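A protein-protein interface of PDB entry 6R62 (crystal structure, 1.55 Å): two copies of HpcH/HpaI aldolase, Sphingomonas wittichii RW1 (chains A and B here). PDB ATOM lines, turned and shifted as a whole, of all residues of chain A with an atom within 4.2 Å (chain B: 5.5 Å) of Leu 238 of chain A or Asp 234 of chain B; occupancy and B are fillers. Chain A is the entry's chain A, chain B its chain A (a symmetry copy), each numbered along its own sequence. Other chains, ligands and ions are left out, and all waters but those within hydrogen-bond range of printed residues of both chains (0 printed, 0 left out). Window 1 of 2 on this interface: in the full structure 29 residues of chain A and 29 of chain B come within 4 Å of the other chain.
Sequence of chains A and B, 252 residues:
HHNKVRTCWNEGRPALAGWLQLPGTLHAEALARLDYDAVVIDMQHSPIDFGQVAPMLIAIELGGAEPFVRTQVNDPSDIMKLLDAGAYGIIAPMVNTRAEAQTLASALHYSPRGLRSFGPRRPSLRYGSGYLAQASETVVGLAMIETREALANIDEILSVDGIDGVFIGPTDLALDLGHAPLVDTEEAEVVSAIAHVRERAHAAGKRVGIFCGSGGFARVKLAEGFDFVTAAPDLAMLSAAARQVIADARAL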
ATOM      1  N   ASP A 234      12.426   7.632   7.732  1.00  0.00           N
ATOM      2  CA  ASP A 234      12.243   9.032   8.091  1.00  0.00           C
ATOM      3  C   ASP A 234      12.670   9.303   9.529  1.00  0.00           C
ATOM      4  O   ASP A 234      13.401  10.268   9.793  1.00  0.00           O
ATOM      5  CB  ASP A 234      10.791   9.480   7.843  1.00  0.00           C
ATOM      6  CG  ASP A 234       9.734   8.571   8.467  1.00  0.00           C
ATOM      7  OD1 ASP A 234      10.046   7.572   9.141  1.00  0.00           O
ATOM      8  OD2 ASP A 234       8.535   8.883   8.274  1.00  0.00           O
ATOM      9  N   LEU A 235      12.255   8.451  10.468  1.00  0.00           N
ATOM     10  CA  LEU A 235      12.585   8.701  11.867  1.00  0.00           C
ATOM     11  C   LEU A 235      14.093   8.651  12.098  1.00  0.00           C
ATOM     12  O   LEU A 235      14.640   9.509  12.805  1.00  0.00           O
ATOM     13  CB  LEU A 235      11.871   7.686  12.754  1.00  0.00           C
ATOM     14  CG  LEU A 235      12.238   7.678  14.228  1.00  0.00           C
ATOM     15  CD1 LEU A 235      11.915   8.994  14.884  1.00  0.00           C
ATOM     16  CD2 LEU A 235      11.510   6.533  14.916  1.00  0.00           C
ATOM     17  N   ALA A 236      14.782   7.657  11.518  1.00  0.00           N
ATOM     18  CA  ALA A 236      16.234   7.557  11.682  1.00  0.00           C
ATOM     19  C   ALA A 236      16.938   8.773  11.090  1.00  0.00           C
ATOM     20  O   ALA A 236      17.846   9.353  11.712  1.00  0.00           O
ATOM     21  CB  ALA A 236      16.763   6.272  11.033  1.00  0.00           C
ATOM     22  N   MET A 237      16.532   9.183   9.887  1.00  0.00           N
ATOM     23  CA  MET A 237      17.170  10.333   9.252  1.00  0.00           C
ATOM     24  C   MET A 237      16.918  11.595  10.060  1.00  0.00           C
ATOM     25  O   MET A 237      17.825  12.410  10.255  1.00  0.00           O
ATOM     26  CB  MET A 237      16.653  10.518   7.826  1.00  0.00           C
ATOM     27  CG  MET A 237      17.021   9.409   6.873  1.00  0.00           C
ATOM     28  SD  MET A 237      16.709   9.850   5.150  1.00  0.00           S
ATOM     29  CE  MET A 237      14.931  10.087   5.117  1.00  0.00           C
ATOM     30  N   LEU A 238      15.682  11.778  10.520  1.00  0.00           N
ATOM     31  CA  LEU A 238      15.337  12.954  11.300  1.00  0.00           C
ATOM     32  C   LEU A 238      16.106  12.988  12.613  1.00  0.00           C
ATOM     33  O   LEU A 238      16.625  14.036  13.010  1.00  0.00           O
ATOM     34  CB  LEU A 238      13.829  12.966  11.549  1.00  0.00           C
ATOM     35  CG  LEU A 238      13.294  14.019  12.514  1.00  0.00           C
ATOM     36  CD1 LEU A 238      13.691  15.450  12.081  1.00  0.00           C
ATOM     37  CD2 LEU A 238      11.794  13.907  12.617  1.00  0.00           C
ATOM     38  N   SER A 239      16.184  11.849  13.305  1.00  0.00           N
ATOM     39  CA  SER A 239      16.892  11.792  14.582  1.00  0.00           C
ATOM     40  C   SER A 239      18.363  12.126  14.411  1.00  0.00           C
ATOM     41  O   SER A 239      18.948  12.859  15.222  1.00  0.00           O
ATOM     42  CB  SER A 239      16.757  10.403  15.203  1.00  0.00           C
ATOM     43  OG  SER A 239      15.419  10.089  15.511  1.00  0.00           O
ATOM     44  N   ALA A 240      18.986  11.577  13.371  1.00  0.00           N
ATOM     45  CA  ALA A 240      20.396  11.852  13.124  1.00  0.00           C
ATOM     46  C   ALA A 240      20.609  13.318  12.794  1.00  0.00           C
ATOM     47  O   ALA A 240      21.578  13.935  13.260  1.00  0.00           O
ATOM     48  CB  ALA A 240      20.908  10.971  11.990  1.00  0.00           C
ATOM     49  N   ALA A 241      19.708  13.900  12.003  1.00  0.00           N
ATOM     50  CA  ALA A 241      19.853  15.308  11.651  1.00  0.00           C
ATOM     51  C   ALA A 241      19.722  16.195  12.880  1.00  0.00           C
ATOM     52  O   ALA A 241      20.478  17.157  13.048  1.00  0.00           O
ATOM     53  CB  ALA A 241      18.812  15.709  10.611  1.00  0.00           C
ATOM     54  N   ALA A 242      18.742  15.906  13.732  1.00  0.00           N
ATOM     55  CA  ALA A 242      18.558  16.677  14.949  1.00  0.00           C
ATOM     56  C   ALA A 242      19.772  16.560  15.859  1.00  0.00           C
ATOM     57  O   ALA A 242      20.220  17.557  16.439  1.00  0.00           O
ATOM     58  CB  ALA A 242      17.284  16.212  15.663  1.00  0.00           C
ATOM     59  N   TRP B  19      11.809  22.103  17.181  1.00  0.00           N
ATOM     60  CA  TRP B  19      10.712  22.788  16.499  1.00  0.00           C
ATOM     61  C   TRP B  19      10.018  21.782  15.601  1.00  0.00           C
ATOM     62  O   TRP B  19      10.644  21.246  14.681  1.00  0.00           O
ATOM     63  CB  TRP B  19      11.223  23.992  15.687  1.00  0.00           C
ATOM     64  CG  TRP B  19      10.131  24.939  15.265  1.00  0.00           C
ATOM     65  CD1 TRP B  19       9.320  24.823  14.170  1.00  0.00           C
ATOM     66  CD2 TRP B  19       9.737  26.138  15.930  1.00  0.00           C
ATOM     67  NE1 TRP B  19       8.437  25.873  14.128  1.00  0.00           N
ATOM     68  CE2 TRP B  19       8.675  26.693  15.197  1.00  0.00           C
ATOM     69  CE3 TRP B  19      10.180  26.799  17.079  1.00  0.00           C
ATOM     70  CZ2 TRP B  19       8.051  27.881  15.578  1.00  0.00           C
ATOM     71  CZ3 TRP B  19       9.558  27.966  17.453  1.00  0.00           C
ATOM     72  CH2 TRP B  19       8.507  28.498  16.703  1.00  0.00           C
ATOM     73  N   LEU B  20       8.733  21.531  15.861  1.00  0.00           N
ATOM     74  CA  LEU B  20       8.000  20.472  15.171  1.00  0.00           C
ATOM     75  C   LEU B  20       6.839  21.054  14.380  1.00  0.00           C
ATOM     76  O   LEU B  20       5.963  21.731  14.950  1.00  0.00           O
ATOM     77  CB  LEU B  20       7.464  19.429  16.161  1.00  0.00           C
ATOM     78  CG  LEU B  20       8.419  18.798  17.161  1.00  0.00           C
ATOM     79  CD1 LEU B  20       7.656  17.771  18.006  1.00  0.00           C
ATOM     80  CD2 LEU B  20       9.576  18.157  16.442  1.00  0.00           C
ATOM     81  N   GLN B  21       6.828  20.778  13.081  1.00  0.00           N
ATOM     82  CA  GLN B  21       5.687  21.046  12.215  1.00  0.00           C
ATOM     83  C   GLN B  21       5.002  19.767  11.755  1.00  0.00           C
ATOM     84  O   GLN B  21       3.956  19.838  11.102  1.00  0.00           O
ATOM     85  CB  GLN B  21       6.129  21.886  11.010  1.00  0.00           C
ATOM     86  CG  GLN B  21       6.554  23.291  11.406  1.00  0.00           C
ATOM     87  CD  GLN B  21       7.413  23.969  10.377  1.00  0.00           C
ATOM     88  OE1 GLN B  21       7.969  23.336   9.482  1.00  0.00           O
ATOM     89  NE2 GLN B  21       7.532  25.292  10.503  1.00  0.00           N
ATOM     90  N   LEU B  22       5.551  18.611  12.084  1.00  0.00           N
ATOM     91  CA  LEU B  22       4.923  17.346  11.733  1.00  0.00           C
ATOM     92  C   LEU B  22       4.146  16.799  12.919  1.00  0.00           C
ATOM     93  O   LEU B  22       4.704  16.684  14.014  1.00  0.00           O
ATOM     94  CB  LEU B  22       5.966  16.333  11.291  1.00  0.00           C
ATOM     95  CG  LEU B  22       6.805  16.785  10.097  1.00  0.00           C
ATOM     96  CD1 LEU B  22       7.898  15.799   9.846  1.00  0.00           C
ATOM     97  CD2 LEU B  22       5.953  16.929   8.829  1.00  0.00           C
ATOM     98  N   HIS B  27       8.304  10.837  16.719  1.00  0.00           N
ATOM     99  CA  HIS B  27       9.432  11.750  16.574  1.00  0.00           C
ATOM    100  C   HIS B  27       9.452  12.805  17.679  1.00  0.00           C
ATOM    101  O   HIS B  27      10.530  13.276  18.056  1.00  0.00           O
ATOM    102  CB  HIS B  27       9.419  12.421  15.202  1.00  0.00           C
ATOM    103  CG  HIS B  27       8.345  13.442  15.031  1.00  0.00           C
ATOM    104  ND1 HIS B  27       7.016  13.169  15.268  1.00  0.00           N
ATOM    105  CD2 HIS B  27       8.399  14.730  14.614  1.00  0.00           C
ATOM    106  CE1 HIS B  27       6.300  14.255  15.022  1.00  0.00           C
ATOM    107  NE2 HIS B  27       7.114  15.211  14.616  1.00  0.00           N
ATOM    108  N   LEU B  31      12.913  13.189  19.646  1.00  0.00           N
ATOM    109  CA  LEU B  31      13.690  14.424  19.683  1.00  0.00           C
ATOM    110  C   LEU B  31      13.784  14.991  21.095  1.00  0.00           C
ATOM    111  O   LEU B  31      14.812  15.585  21.458  1.00  0.00           O
ATOM    112  CB  LEU B  31      13.103  15.460  18.719  1.00  0.00           C
ATOM    113  CG  LEU B  31      13.749  15.427  17.324  1.00  0.00           C
ATOM    114  CD1 LEU B  31      13.789  14.022  16.750  1.00  0.00           C
ATOM    115  CD2 LEU B  31      12.993  16.337  16.379  1.00  0.00           C
ATOM    116  N   ALA B 232      16.271  22.722  14.474  1.00  0.00           N
ATOM    117  CA  ALA B 232      15.637  23.411  13.352  1.00  0.00           C
ATOM    118  C   ALA B 232      14.361  22.605  13.060  1.00  0.00           C
ATOM    119  O   ALA B 232      14.177  21.538  13.644  1.00  0.00           O
ATOM    120  CB  ALA B 232      16.566  23.468  12.139  1.00  0.00           C
ATOM    121  N   PRO B 233      13.457  23.108  12.216  1.00  0.00           N
ATOM    122  CA  PRO B 233      12.177  22.407  12.018  1.00  0.00           C
ATOM    123  C   PRO B 233      12.358  20.965  11.578  1.00  0.00           C
ATOM    124  O   PRO B 233      13.175  20.658  10.703  1.00  0.00           O
ATOM    125  CB  PRO B 233      11.480  23.231  10.937  1.00  0.00           C
ATOM    126  CG  PRO B 233      12.046  24.593  11.118  1.00  0.00           C
ATOM    127  CD  PRO B 233      13.485  24.388  11.488  1.00  0.00           C
ATOM    128  N   ASP B 234      11.538  20.087  12.155  1.00  0.00           N
ATOM    129  CA  ASP B 234      11.624  18.671  11.818  1.00  0.00           C
ATOM    130  C   ASP B 234      11.469  18.441  10.318  1.00  0.00           C
ATOM    131  O   ASP B 234      12.263  17.707   9.713  1.00  0.00           O
ATOM    132  CB  ASP B 234      10.598  17.851  12.620  1.00  0.00           C
ATOM    133  CG  ASP B 234       9.169  18.384  12.552  1.00  0.00           C
ATOM    134  OD1 ASP B 234       8.876  19.387  11.874  1.00  0.00           O
ATOM    135  OD2 ASP B 234       8.301  17.761  13.207  1.00  0.00           O
ATOM    136  N   LEU B 235      10.479  19.082   9.694  1.00  0.00           N
ATOM    137  CA  LEU B 235      10.250  18.848   8.272  1.00  0.00           C
ATOM    138  C   LEU B 235      11.443  19.303   7.437  1.00  0.00           C
ATOM    139  O   LEU B 235      11.864  18.592   6.514  1.00  0.00           O
ATOM    140  CB  LEU B 235       8.979  19.563   7.830  1.00  0.00           C
ATOM    141  CG  LEU B 235       8.678  19.580   6.341  1.00  0.00           C
ATOM    142  CD1 LEU B 235       8.495  18.189   5.798  1.00  0.00           C
ATOM    143  CD2 LEU B 235       7.440  20.430   6.093  1.00  0.00           C
ATOM    144  N   ALA B 236      12.001  20.487   7.738  1.00  0.00           N
ATOM    145  CA  ALA B 236      13.160  20.980   6.990  1.00  0.00           C
ATOM    146  C   ALA B 236      14.359  20.050   7.156  1.00  0.00           C
ATOM    147  O   ALA B 236      15.046  19.711   6.176  1.00  0.00           O
ATOM    148  CB  ALA B 236      13.528  22.400   7.437  1.00  0.00           C
ATOM    149  N   MET B 237      14.623  19.620   8.390  1.00  0.00           N
ATOM    150  CA  MET B 237      15.762  18.738   8.627  1.00  0.00           C
ATOM    151  C   MET B 237      15.563  17.408   7.921  1.00  0.00           C
ATOM    152  O   MET B 237      16.494  16.869   7.313  1.00  0.00           O
ATOM    153  CB  MET B 237      15.964  18.504  10.124  1.00  0.00           C
ATOM    154  CG  MET B 237      16.368  19.730  10.904  1.00  0.00           C
ATOM    155  SD  MET B 237      16.941  19.328  12.569  1.00  0.00           S
ATOM    156  CE  MET B 237      15.484  18.605  13.326  1.00  0.00           C
ATOM    157  N   LEU B 238      14.355  16.856   8.007  1.00  0.00           N
ATOM    158  CA  LEU B 238      14.061  15.583   7.371  1.00  0.00           C
ATOM    159  C   LEU B 238      14.187  15.684   5.856  1.00  0.00           C
ATOM    160  O   LEU B 238      14.764  14.801   5.215  1.00  0.00           O
ATOM    161  CB  LEU B 238      12.657  15.133   7.772  1.00  0.00           C
ATOM    162  CG  LEU B 238      12.088  13.914   7.056  1.00  0.00           C
ATOM    163  CD1 LEU B 238      13.014  12.681   7.191  1.00  0.00           C
ATOM    164  CD2 LEU B 238      10.716  13.593   7.595  1.00  0.00           C
ATOM    165  N   SER B 239      13.646  16.752   5.269  1.00  0.00           N
ATOM    166  CA  SER B 239      13.710  16.927   3.818  1.00  0.00           C
ATOM    167  C   SER B 239      15.145  17.031   3.338  1.00  0.00           C
ATOM    168  O   SER B 239      15.519  16.442   2.315  1.00  0.00           O
ATOM    169  CB  SER B 239      12.943  18.181   3.400  1.00  0.00           C
ATOM    170  OG  SER B 239      11.569  18.085   3.699  1.00  0.00           O
ATOM    171  N   ALA B 241      17.812  15.861   4.849  1.00  0.00           N
ATOM    172  CA  ALA B 241      18.479  14.576   5.020  1.00  0.00           C
ATOM    173  C   ALA B 241      18.103  13.613   3.905  1.00  0.00           C
ATOM    174  O   ALA B 241      18.955  12.893   3.376  1.00  0.00           O
ATOM    175  CB  ALA B 241      18.126  13.964   6.372  1.00  0.00           C
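The backbone carbonyl oxygen (O) of Trp 19 of chain B sits at hydrogen-bond distance from the backbone NH (N) of Asp 234 of chain B (2.9 Å).
OD1 of Asp 234 of chain B is in hydrogen-bond range of N of Gln 21 of chain B (2.8 Å).
NE2 of His 27 of chain B lies within hydrogen-bond range of O of Leu 22 of chain B (2.9 Å).
The backbone NH (N) of Leu 22 of chain B lies within hydrogen-bond range of the side-chain carboxylate (OD2) of Asp 234 of chain B (3.1 Å).
OD2 of Asp 234 of chain B lies within hydrogen-bond range of NE2 of His 27 of chain B, at 3.1 Å.
Asp 234 of chain A touches Leu 238 of chain B, and with the chains exchanged Leu 238 of chain A touches Asp 234 of chain B.
Met 237 of chain A touches Leu 238 of chain B, and with the chains exchanged Leu 238 of chain A touches Met 237 of chain B.
7 positions are printed for both chains.
Of the 7 pairs that touch across the chains among the printed residues, 4 have their exchanged pair printed and touching as well.
Leu 238 of chain A touches three residues of chain B.
Printed residues of chain A within 4 Å of Asp 234 of chain B: Leu 238.
Printed residues of chain B within 4 Å of Ala 242 of chain A: Leu 31 (3.98 Å) and Met 237 (3.8 Å).
Printed residues of chain A within 4 Å of Met 237 of chain B: Leu 238 and Ala 242.
Of the printed residues of chain B, Asp 234 of chain A touches Leu 238.
Of the printed residues of chain A, Leu 238 of chain B touches Asp 234 (3.6 Å) and Met 237 (3.8 Å).
The nearest printed residue of chain A that does not touch Asp 234 of chain B is Ala 241 of chain A (6.9 Å).
The nearest printed residue of chain A that does not touch Leu 238 of chain B is Leu 238 of chain A (4.4 Å).
Leu 238 of chain B touches Asp 234 of chain A.
Met 237 of chain A touches Leu 238 of chain B (CE to CD1, 3.8 Å).
His 27 of chain B touches Leu 238 of chain A.
Asp 234 of chain B touches Leu 238 of chain A.
Met 237 of chain B touches Leu 238 of chain A (CE to CD1, 3.8 Å).
CG of Leu 31 of chain B touches CB of Ala 242 of chain A, at 3.98 Å.
Met 237 of chain B touches Ala 242 of chain A.
Hydrophobic or aromatic side chains of chain A that line the printed part of chain B: Met 237, Leu 238 and Ala 242.
Along chain A the printed residues that touch a printed residue of chain B span positions 234 to 242.
Printed residues of chain B that touch a printed residue of chain A: His 27, Leu 31, Asp 234, Met 237 and Leu 238.
Hydrophobic or aromatic side chains of chain B that line the printed part of chain A: His 27, Leu 31, Met 237 and Leu 238.
Among the printed residues, 7 pairs touch across the chains.
Among the printed residues, no Asp or Glu carboxylate lies within 4 Å of a Lys or Arg side-chain nitrogen of the other chain.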
